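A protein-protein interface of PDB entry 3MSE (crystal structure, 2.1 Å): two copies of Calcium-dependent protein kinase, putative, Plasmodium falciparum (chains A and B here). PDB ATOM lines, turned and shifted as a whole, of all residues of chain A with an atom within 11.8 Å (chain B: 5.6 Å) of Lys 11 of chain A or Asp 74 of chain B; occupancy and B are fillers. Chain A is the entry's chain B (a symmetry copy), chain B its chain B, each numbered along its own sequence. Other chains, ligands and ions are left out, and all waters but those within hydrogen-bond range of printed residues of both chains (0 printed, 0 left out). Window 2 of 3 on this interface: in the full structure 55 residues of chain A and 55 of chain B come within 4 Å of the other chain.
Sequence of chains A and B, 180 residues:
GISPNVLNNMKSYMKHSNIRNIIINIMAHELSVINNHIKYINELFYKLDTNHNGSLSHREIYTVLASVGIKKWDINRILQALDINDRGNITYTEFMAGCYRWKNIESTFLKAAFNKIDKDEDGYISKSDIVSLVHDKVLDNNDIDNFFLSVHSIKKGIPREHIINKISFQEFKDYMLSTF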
ATOM      1  N   ILE A   2      -5.006 -13.199   2.826  1.00  0.00           N
ATOM      2  CA  ILE A   2      -5.095 -12.368   1.583  1.00  0.00           C
ATOM      3  C   ILE A   2      -5.527 -13.201   0.381  1.00  0.00           C
ATOM      4  O   ILE A   2      -4.971 -14.272   0.139  1.00  0.00           O
ATOM      5  CB  ILE A   2      -3.757 -11.723   1.234  1.00  0.00           C
ATOM      6  CG1 ILE A   2      -3.210 -10.958   2.435  1.00  0.00           C
ATOM      7  CG2 ILE A   2      -3.897 -10.835  -0.015  1.00  0.00           C
ATOM      8  CD1 ILE A   2      -1.819 -10.460   2.233  1.00  0.00           C
ATOM      9  N   SER A   3      -6.488 -12.688  -0.386  1.00  0.00           N
ATOM     10  CA  SER A   3      -6.999 -13.397  -1.557  1.00  0.00           C
ATOM     11  C   SER A   3      -5.917 -13.592  -2.612  1.00  0.00           C
ATOM     12  O   SER A   3      -5.119 -12.676  -2.871  1.00  0.00           O
ATOM     13  CB  SER A   3      -8.199 -12.673  -2.166  1.00  0.00           C
ATOM     14  OG  SER A   3      -7.848 -12.042  -3.390  1.00  0.00           O
ATOM     15  N   PRO A   4      -5.895 -14.786  -3.240  1.00  0.00           N
ATOM     16  CA  PRO A   4      -4.855 -15.114  -4.198  1.00  0.00           C
ATOM     17  C   PRO A   4      -4.796 -14.163  -5.393  1.00  0.00           C
ATOM     18  O   PRO A   4      -3.725 -13.980  -5.983  1.00  0.00           O
ATOM     19  CB  PRO A   4      -5.244 -16.527  -4.666  1.00  0.00           C
ATOM     20  CG  PRO A   4      -5.985 -17.105  -3.504  1.00  0.00           C
ATOM     21  CD  PRO A   4      -6.773 -15.946  -2.964  1.00  0.00           C
ATOM     22  N   ASN A   5      -5.934 -13.576  -5.767  1.00  0.00           N
ATOM     23  CA  ASN A   5      -5.964 -12.640  -6.897  1.00  0.00           C
ATOM     24  C   ASN A   5      -5.165 -11.361  -6.621  1.00  0.00           C
ATOM     25  O   ASN A   5      -4.492 -10.841  -7.509  1.00  0.00           O
ATOM     26  CB  ASN A   5      -7.401 -12.328  -7.350  1.00  0.00           C
ATOM     27  CG  ASN A   5      -7.868 -10.938  -6.951  1.00  0.00           C
ATOM     28  OD1 ASN A   5      -7.748  -9.976  -7.728  1.00  0.00           O
ATOM     29  ND2 ASN A   5      -8.428 -10.824  -5.749  1.00  0.00           N
ATOM     30  N   VAL A   6      -5.220 -10.885  -5.378  1.00  0.00           N
ATOM     31  CA  VAL A   6      -4.439  -9.708  -4.962  1.00  0.00           C
ATOM     32  C   VAL A   6      -2.942 -10.046  -4.939  1.00  0.00           C
ATOM     33  O   VAL A   6      -2.103  -9.264  -5.409  1.00  0.00           O
ATOM     34  CB  VAL A   6      -4.917  -9.138  -3.598  1.00  0.00           C
ATOM     35  CG1 VAL A   6      -3.940  -8.085  -3.066  1.00  0.00           C
ATOM     36  CG2 VAL A   6      -6.321  -8.518  -3.758  1.00  0.00           C
ATOM     37  N   LEU A   7      -2.622 -11.243  -4.444  1.00  0.00           N
ATOM     38  CA  LEU A   7      -1.238 -11.725  -4.439  1.00  0.00           C
ATOM     39  C   LEU A   7      -0.662 -11.863  -5.830  1.00  0.00           C
ATOM     40  O   LEU A   7       0.466 -11.418  -6.092  1.00  0.00           O
ATOM     41  CB  LEU A   7      -1.129 -13.039  -3.663  1.00  0.00           C
ATOM     42  CG  LEU A   7      -1.449 -12.909  -2.182  1.00  0.00           C
ATOM     43  CD1 LEU A   7      -1.374 -14.286  -1.506  1.00  0.00           C
ATOM     44  CD2 LEU A   7      -0.509 -11.879  -1.499  1.00  0.00           C
ATOM     45  N   ASN A   8      -1.447 -12.448  -6.728  1.00  0.00           N
ATOM     46  CA  ASN A   8      -1.058 -12.584  -8.127  1.00  0.00           C
ATOM     47  C   ASN A   8      -0.940 -11.228  -8.836  1.00  0.00           C
ATOM     48  O   ASN A   8      -0.102 -11.051  -9.729  1.00  0.00           O
ATOM     49  CB  ASN A   8      -2.073 -13.466  -8.870  1.00  0.00           C
ATOM     50  CG  ASN A   8      -1.939 -14.958  -8.516  1.00  0.00           C
ATOM     51  OD1 ASN A   8      -0.837 -15.456  -8.241  1.00  0.00           O
ATOM     52  ND2 ASN A   8      -3.060 -15.671  -8.544  1.00  0.00           N
ATOM     53  N   ASN A   9      -1.802 -10.286  -8.456  1.00  0.00           N
ATOM     54  CA  ASN A   9      -1.725  -8.921  -9.008  1.00  0.00           C
ATOM     55  C   ASN A   9      -0.382  -8.303  -8.619  1.00  0.00           C
ATOM     56  O   ASN A   9       0.322  -7.800  -9.459  1.00  0.00           O
ATOM     57  CB  ASN A   9      -2.886  -8.026  -8.512  1.00  0.00           C
ATOM     58  CG  ASN A   9      -4.246  -8.418  -9.094  1.00  0.00           C
ATOM     59  OD1 ASN A   9      -4.329  -9.003 -10.171  1.00  0.00           O
ATOM     60  ND2 ASN A   9      -5.330  -8.064  -8.379  1.00  0.00           N
ATOM     61  N   MET A  10      -0.019  -8.392  -7.347  1.00  0.00           N
ATOM     62  CA  MET A  10       1.286  -7.887  -6.891  1.00  0.00           C
ATOM     63  C   MET A  10       2.462  -8.519  -7.643  1.00  0.00           C
ATOM     64  O   MET A  10       3.411  -7.826  -8.042  1.00  0.00           O
ATOM     65  CB  MET A  10       1.467  -8.120  -5.394  1.00  0.00           C
ATOM     66  CG  MET A  10       0.502  -7.385  -4.516  1.00  0.00           C
ATOM     67  SD  MET A  10       0.799  -7.880  -2.825  1.00  0.00           S
ATOM     68  CE  MET A  10      -0.412  -6.969  -1.875  1.00  0.00           C
ATOM     69  N   LYS A  11       2.397  -9.838  -7.834  1.00  0.00           N
ATOM     70  CA  LYS A  11       3.476 -10.559  -8.526  1.00  0.00           C
ATOM     71  C   LYS A  11       3.601 -10.171  -9.973  1.00  0.00           C
ATOM     72  O   LYS A  11       4.696 -10.182 -10.532  1.00  0.00           O
ATOM     73  CB  LYS A  11       3.285 -12.071  -8.417  1.00  0.00           C
ATOM     74  CG  LYS A  11       3.641 -12.653  -7.063  1.00  0.00           C
ATOM     75  CD  LYS A  11       2.853 -13.971  -6.877  1.00  0.00           C
ATOM     76  CE  LYS A  11       3.487 -14.909  -5.879  1.00  0.00           C
ATOM     77  NZ  LYS A  11       4.343 -15.941  -6.581  1.00  0.00           N
ATOM     78  N   SER A  12       2.488  -9.840 -10.609  1.00  0.00           N
ATOM     79  CA  SER A  12       2.566  -9.345 -11.971  1.00  0.00           C
ATOM     80  C   SER A  12       3.069  -7.886 -11.997  1.00  0.00           C
ATOM     81  O   SER A  12       3.859  -7.506 -12.859  1.00  0.00           O
ATOM     82  CB  SER A  12       1.215  -9.478 -12.666  1.00  0.00           C
ATOM     83  OG  SER A  12       1.164  -8.630 -13.788  1.00  0.00           O
ATOM     84  N   TYR A  13       2.623  -7.086 -11.030  1.00  0.00           N
ATOM     85  CA  TYR A  13       3.032  -5.672 -10.932  1.00  0.00           C
ATOM     86  C   TYR A  13       4.548  -5.534 -10.792  1.00  0.00           C
ATOM     87  O   TYR A  13       5.169  -4.695 -11.455  1.00  0.00           O
ATOM     88  CB  TYR A  13       2.326  -5.050  -9.726  1.00  0.00           C
ATOM     89  CG  TYR A  13       2.456  -3.542  -9.559  1.00  0.00           C
ATOM     90  CD1 TYR A  13       1.687  -2.663 -10.328  1.00  0.00           C
ATOM     91  CD2 TYR A  13       3.269  -3.007  -8.574  1.00  0.00           C
ATOM     92  CE1 TYR A  13       1.762  -1.281 -10.137  1.00  0.00           C
ATOM     93  CE2 TYR A  13       3.361  -1.627  -8.382  1.00  0.00           C
ATOM     94  CZ  TYR A  13       2.588  -0.776  -9.166  1.00  0.00           C
ATOM     95  OH  TYR A  13       2.685   0.585  -8.980  1.00  0.00           O
ATOM     96  N   MET A  14       5.143  -6.390  -9.954  1.00  0.00           N
ATOM     97  CA  MET A  14       6.583  -6.341  -9.666  1.00  0.00           C
ATOM     98  C   MET A  14       7.456  -6.545 -10.906  1.00  0.00           C
ATOM     99  O   MET A  14       8.610  -6.160 -10.905  1.00  0.00           O
ATOM    100  CB  MET A  14       6.949  -7.350  -8.560  1.00  0.00           C
ATOM    101  CG  MET A  14       7.228  -8.807  -9.059  1.00  0.00           C
ATOM    102  SD  MET A  14       7.364  -9.997  -7.700  1.00  0.00           S
ATOM    103  CE  MET A  14       7.613 -11.512  -8.647  1.00  0.00           C
ATOM    104  N   LYS A  15       6.904  -7.140 -11.963  1.00  0.00           N
ATOM    105  CA  LYS A  15       7.677  -7.442 -13.166  1.00  0.00           C
ATOM    106  C   LYS A  15       7.742  -6.277 -14.161  1.00  0.00           C
ATOM    107  O   LYS A  15       8.514  -6.310 -15.104  1.00  0.00           O
ATOM    108  CB  LYS A  15       7.139  -8.719 -13.847  1.00  0.00           C
ATOM    109  CG  LYS A  15       7.464 -10.034 -13.074  1.00  0.00           C
ATOM    110  CD  LYS A  15       6.921 -11.263 -13.842  1.00  0.00           C
ATOM    111  CE  LYS A  15       6.974 -12.542 -13.008  1.00  0.00           C
ATOM    112  NZ  LYS A  15       6.158 -12.410 -11.776  1.00  0.00           N
ATOM    113  N   HIS A  16       6.941  -5.239 -13.948  1.00  0.00           N
ATOM    114  CA  HIS A  16       6.905  -4.151 -14.908  1.00  0.00           C
ATOM    115  C   HIS A  16       7.844  -3.006 -14.534  1.00  0.00           C
ATOM    116  O   HIS A  16       8.379  -2.966 -13.411  1.00  0.00           O
ATOM    117  CB  HIS A  16       5.457  -3.712 -15.154  1.00  0.00           C
ATOM    118  CG  HIS A  16       4.677  -4.728 -15.923  1.00  0.00           C
ATOM    119  ND1 HIS A  16       4.890  -4.956 -17.266  1.00  0.00           N
ATOM    120  CD2 HIS A  16       3.753  -5.637 -15.528  1.00  0.00           C
ATOM    121  CE1 HIS A  16       4.098  -5.934 -17.675  1.00  0.00           C
ATOM    122  NE2 HIS A  16       3.398  -6.363 -16.639  1.00  0.00           N
ATOM    123  N   SER A  17       8.080  -2.102 -15.478  1.00  0.00           N
ATOM    124  CA  SER A  17       9.006  -0.992 -15.264  1.00  0.00           C
ATOM    125  C   SER A  17       8.437   0.045 -14.302  1.00  0.00           C
ATOM    126  O   SER A  17       7.224   0.107 -14.079  1.00  0.00           O
ATOM    127  CB  SER A  17       9.356  -0.328 -16.594  1.00  0.00           C
ATOM    128  OG  SER A  17       8.214   0.287 -17.184  1.00  0.00           O
ATOM    129  N   ARG A  20       5.985   2.310 -16.332  1.00  0.00           N
ATOM    130  CA  ARG A  20       4.675   1.646 -16.480  1.00  0.00           C
ATOM    131  C   ARG A  20       3.863   1.790 -15.207  1.00  0.00           C
ATOM    132  O   ARG A  20       2.677   2.133 -15.240  1.00  0.00           O
ATOM    133  CB  ARG A  20       4.874   0.152 -16.780  1.00  0.00           C
ATOM    134  CG  ARG A  20       3.778  -0.509 -17.582  1.00  0.00           C
ATOM    135  CD  ARG A  20       2.498  -0.859 -16.839  1.00  0.00           C
ATOM    136  NE  ARG A  20       2.657  -1.584 -15.583  1.00  0.00           N
ATOM    137  CZ  ARG A  20       1.905  -2.626 -15.195  1.00  0.00           C
ATOM    138  NH1 ARG A  20       0.970  -3.129 -15.985  1.00  0.00           N
ATOM    139  NH2 ARG A  20       2.114  -3.186 -14.014  1.00  0.00           N
ATOM    140  N   ASN A  21       4.504   1.526 -14.079  1.00  0.00           N
ATOM    141  CA  ASN A  21       3.799   1.553 -12.814  1.00  0.00           C
ATOM    142  C   ASN A  21       3.464   2.983 -12.352  1.00  0.00           C
ATOM    143  O   ASN A  21       2.460   3.195 -11.700  1.00  0.00           O
ATOM    144  CB  ASN A  21       4.585   0.771 -11.762  1.00  0.00           C
ATOM    145  CG  ASN A  21       4.580  -0.747 -12.044  1.00  0.00           C
ATOM    146  OD1 ASN A  21       3.830  -1.218 -12.894  1.00  0.00           O
ATOM    147  ND2 ASN A  21       5.417  -1.490 -11.340  1.00  0.00           N
ATOM    148  N   THR A 179       0.433  -4.978 -21.299  1.00  0.00           N
ATOM    149  CA  THR A 179       1.139  -5.206 -20.037  1.00  0.00           C
ATOM    150  C   THR A 179       0.184  -5.695 -18.976  1.00  0.00           C
ATOM    151  O   THR A 179       0.602  -6.088 -17.887  1.00  0.00           O
ATOM    152  CB  THR A 179       1.867  -3.935 -19.498  1.00  0.00           C
ATOM    153  OG1 THR A 179       0.909  -2.992 -18.998  1.00  0.00           O
ATOM    154  CG2 THR A 179       2.738  -3.296 -20.565  1.00  0.00           C
ATOM    155  N   PHE A 180      -1.108  -5.656 -19.291  1.00  0.00           N
ATOM    156  CA  PHE A 180      -2.124  -6.164 -18.378  1.00  0.00           C
ATOM    157  C   PHE A 180      -2.246  -7.689 -18.507  1.00  0.00           C
ATOM    158  O   PHE A 180      -3.147  -8.296 -17.934  1.00  0.00           O
ATOM    159  CB  PHE A 180      -3.490  -5.507 -18.638  1.00  0.00           C
ATOM    160  CG  PHE A 180      -3.500  -4.001 -18.496  1.00  0.00           C
ATOM    161  CD1 PHE A 180      -2.615  -3.346 -17.640  1.00  0.00           C
ATOM    162  CD2 PHE A 180      -4.430  -3.242 -19.201  1.00  0.00           C
ATOM    163  CE1 PHE A 180      -2.642  -1.947 -17.514  1.00  0.00           C
ATOM    164  CE2 PHE A 180      -4.470  -1.838 -19.070  1.00  0.00           C
ATOM    165  CZ  PHE A 180      -3.572  -1.197 -18.231  1.00  0.00           C
ATOM    166  OXT PHE A 180      -1.454  -8.364 -19.184  1.00  0.00           O
ATOM    167  N   ILE B  70       4.408 -15.815   0.503  1.00  0.00           N
ATOM    168  CA  ILE B  70       5.267 -15.169  -0.489  1.00  0.00           C
ATOM    169  C   ILE B  70       6.709 -15.253   0.008  1.00  0.00           C
ATOM    170  O   ILE B  70       6.969 -15.003   1.177  1.00  0.00           O
ATOM    171  CB  ILE B  70       4.859 -13.684  -0.728  1.00  0.00           C
ATOM    172  CG1 ILE B  70       3.335 -13.572  -0.896  1.00  0.00           C
ATOM    173  CG2 ILE B  70       5.656 -13.075  -1.901  1.00  0.00           C
ATOM    174  CD1 ILE B  70       2.743 -14.417  -2.035  1.00  0.00           C
ATOM    175  N   LYS B  71       7.639 -15.593  -0.878  1.00  0.00           N
ATOM    176  CA  LYS B  71       9.034 -15.775  -0.482  1.00  0.00           C
ATOM    177  C   LYS B  71       9.799 -14.446  -0.499  1.00  0.00           C
ATOM    178  O   LYS B  71       9.465 -13.527  -1.261  1.00  0.00           O
ATOM    179  CB  LYS B  71       9.727 -16.795  -1.407  1.00  0.00           C
ATOM    180  CG  LYS B  71       9.091 -18.201  -1.360  1.00  0.00           C
ATOM    181  CD  LYS B  71       9.414 -18.898  -0.027  1.00  0.00           C
ATOM    182  CE  LYS B  71       8.712 -20.257   0.115  1.00  0.00           C
ATOM    183  NZ  LYS B  71       8.932 -20.742   1.506  1.00  0.00           N
ATOM    184  N   LYS B  72      10.833 -14.379   0.335  1.00  0.00           N
ATOM    185  CA  LYS B  72      11.671 -13.204   0.504  1.00  0.00           C
ATOM    186  C   LYS B  72      12.010 -12.496  -0.813  1.00  0.00           C
ATOM    187  O   LYS B  72      11.846 -11.285  -0.912  1.00  0.00           O
ATOM    188  CB  LYS B  72      12.966 -13.579   1.235  1.00  0.00           C
ATOM    189  CG  LYS B  72      14.017 -12.471   1.224  1.00  0.00           C
ATOM    190  CD  LYS B  72      15.097 -12.697   2.276  1.00  0.00           C
ATOM    191  CE  LYS B  72      16.211 -11.674   2.090  1.00  0.00           C
ATOM    192  NZ  LYS B  72      17.142 -11.681   3.249  1.00  0.00           N
ATOM    193  N   TRP B  73      12.481 -13.245  -1.807  1.00  0.00           N
ATOM    194  CA  TRP B  73      12.890 -12.651  -3.081  1.00  0.00           C
ATOM    195  C   TRP B  73      11.712 -12.024  -3.817  1.00  0.00           C
ATOM    196  O   TRP B  73      11.872 -11.000  -4.458  1.00  0.00           O
ATOM    197  CB  TRP B  73      13.605 -13.654  -3.981  1.00  0.00           C
ATOM    198  CG  TRP B  73      12.990 -15.034  -3.956  1.00  0.00           C
ATOM    199  CD1 TRP B  73      12.066 -15.538  -4.819  1.00  0.00           C
ATOM    200  CD2 TRP B  73      13.292 -16.088  -3.025  1.00  0.00           C
ATOM    201  NE1 TRP B  73      11.762 -16.842  -4.483  1.00  0.00           N
ATOM    202  CE2 TRP B  73      12.502 -17.205  -3.387  1.00  0.00           C
ATOM    203  CE3 TRP B  73      14.155 -16.195  -1.926  1.00  0.00           C
ATOM    204  CZ2 TRP B  73      12.539 -18.423  -2.681  1.00  0.00           C
ATOM    205  CZ3 TRP B  73      14.193 -17.411  -1.214  1.00  0.00           C
ATOM    206  CH2 TRP B  73      13.377 -18.502  -1.595  1.00  0.00           C
ATOM    207  N   ASP B  74      10.531 -12.615  -3.700  1.00  0.00           N
ATOM    208  CA  ASP B  74       9.356 -11.993  -4.283  1.00  0.00           C
ATOM    209  C   ASP B  74       8.902 -10.758  -3.484  1.00  0.00           C
ATOM    210  O   ASP B  74       8.591  -9.711  -4.073  1.00  0.00           O
ATOM    211  CB  ASP B  74       8.228 -13.007  -4.462  1.00  0.00           C
ATOM    212  CG  ASP B  74       8.517 -14.010  -5.597  1.00  0.00           C
ATOM    213  OD1 ASP B  74       9.324 -13.706  -6.510  1.00  0.00           O
ATOM    214  OD2 ASP B  74       7.915 -15.101  -5.576  1.00  0.00           O
ATOM    215  N   ILE B  75       8.868 -10.888  -2.159  1.00  0.00           N
ATOM    216  CA  ILE B  75       8.416  -9.796  -1.293  1.00  0.00           C
ATOM    217  C   ILE B  75       9.253  -8.544  -1.600  1.00  0.00           C
ATOM    218  O   ILE B  75       8.703  -7.462  -1.791  1.00  0.00           O
ATOM    219  CB  ILE B  75       8.521 -10.125   0.214  1.00  0.00           C
ATOM    220  CG1 ILE B  75       7.639 -11.321   0.605  1.00  0.00           C
ATOM    221  CG2 ILE B  75       8.114  -8.886   1.074  1.00  0.00           C
ATOM    222  CD1 ILE B  75       7.789 -11.695   2.063  1.00  0.00           C
ATOM    223  N   ASN B  76      10.573  -8.707  -1.668  1.00  0.00           N
ATOM    224  CA  ASN B  76      11.456  -7.577  -1.972  1.00  0.00           C
ATOM    225  C   ASN B  76      11.230  -6.937  -3.345  1.00  0.00           C
ATOM    226  O   ASN B  76      11.301  -5.695  -3.464  1.00  0.00           O
ATOM    227  CB  ASN B  76      12.920  -7.944  -1.757  1.00  0.00           C
ATOM    228  CG  ASN B  76      13.298  -7.986  -0.272  1.00  0.00           C
ATOM    229  OD1 ASN B  76      12.643  -7.375   0.578  1.00  0.00           O
ATOM    230  ND2 ASN B  76      14.346  -8.718   0.036  1.00  0.00           N
ATOM    231  N   ARG B  77      10.952  -7.749  -4.372  1.00  0.00           N
ATOM    232  CA  ARG B  77      10.606  -7.177  -5.675  1.00  0.00           C
ATOM    233  C   ARG B  77       9.271  -6.432  -5.643  1.00  0.00           C
ATOM    234  O   ARG B  77       9.140  -5.411  -6.309  1.00  0.00           O
ATOM    235  CB  ARG B  77      10.591  -8.214  -6.797  1.00  0.00           C
ATOM    236  CG  ARG B  77      11.957  -8.848  -7.066  1.00  0.00           C
ATOM    237  CD  ARG B  77      11.820  -9.976  -8.076  1.00  0.00           C
ATOM    238  NE  ARG B  77      11.510  -9.463  -9.402  1.00  0.00           N
ATOM    239  CZ  ARG B  77      11.190 -10.225 -10.443  1.00  0.00           C
ATOM    240  NH1 ARG B  77      11.141 -11.552 -10.317  1.00  0.00           N
ATOM    241  NH2 ARG B  77      10.940  -9.660 -11.620  1.00  0.00           N
ATOM    242  N   ILE B  78       8.303  -6.960  -4.886  1.00  0.00           N
ATOM    243  CA  ILE B  78       7.003  -6.318  -4.708  1.00  0.00           C
ATOM    244  C   ILE B  78       7.191  -4.965  -3.989  1.00  0.00           C
ATOM    245  O   ILE B  78       6.666  -3.940  -4.418  1.00  0.00           O
ATOM    246  CB  ILE B  78       6.025  -7.228  -3.956  1.00  0.00           C
ATOM    247  CG1 ILE B  78       5.589  -8.396  -4.856  1.00  0.00           C
ATOM    248  CG2 ILE B  78       4.798  -6.453  -3.470  1.00  0.00           C
ATOM    249  CD1 ILE B  78       4.918  -9.519  -4.086  1.00  0.00           C
ATOM    250  N   LEU B  79       7.992  -4.973  -2.939  1.00  0.00           N
ATOM    251  CA  LEU B  79       8.268  -3.778  -2.173  1.00  0.00           C
ATOM    252  C   LEU B  79       8.881  -2.666  -3.020  1.00  0.00           C
ATOM    253  O   LEU B  79       8.408  -1.536  -2.961  1.00  0.00           O
ATOM    254  CB  LEU B  79       9.131  -4.101  -0.951  1.00  0.00           C
ATOM    255  CG  LEU B  79       8.366  -4.725   0.214  1.00  0.00           C
ATOM    256  CD1 LEU B  79       9.338  -5.020   1.377  1.00  0.00           C
ATOM    257  CD2 LEU B  79       7.217  -3.818   0.693  1.00  0.00           C
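The side-chain carboxylate (OD2) of Asp 74 of chain B lies within salt-bridge range of the side-chain amino group (NZ) of Lys 11 of chain A, at 3.8 Å.
The backbone carbonyl oxygen (O) of Lys 11 of chain A sits at hydrogen-bond distance from the side-chain amino group (NZ) of Lys 15 of chain A (2.9 Å).
O of Met 10 of chain A touches CG1 of Ile 78 of chain B, 3.9 Å away.
CD1 of Ile 70 of chain B touches CE of Lys 11 of chain A (3.9 Å).
OD1 of Asp 74 of chain B touches CE of Met 14 of chain A (3.5 Å).
Met 14 of chain A touches Arg 77 of chain B (CB to O, 3.7 Å).
CG1 of Ile 78 of chain B touches SD of Met 14 of chain A (3.7 Å).
NH2 of Arg 77 of chain B touches CG of Lys 15 of chain A, 3.8 Å away.
Printed residues of chain B within 4 Å of Met 10 of chain A: Ile 78 (3.9 Å).
Lys 11 of chain A touches two residues of chain B.
Printed residues of chain B within 4 Å of Lys 15 of chain A: Arg 77.
Of chain A, only Lys 11 (3.9 Å) comes within 4 Å of Ile 70 of chain B.
Asp 74 of chain B touches just these residues of chain A: Lys 11 (3.8 Å) and Met 14 (3.5 Å).
No residue of chain A comes within 4 Å of Asn 76 of chain B.
Of chain A, only Met 10 and Met 14 come within 4 Å of Ile 78 of chain B.
The nearest printed residue of chain B that does not touch Met 14 of chain A is Trp 73 of chain B (5.6 Å).
Hydrophobic or aromatic side chains of chain A that line the printed part of chain B: Met 10 and Met 14.
Along chain B the printed residues that touch a printed residue of chain A span positions 70 to 78.
No position is printed for both chains.
Of the 7 pairs that touch across the chains among the printed residues, none has its exchanged pair printed and touching as well.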
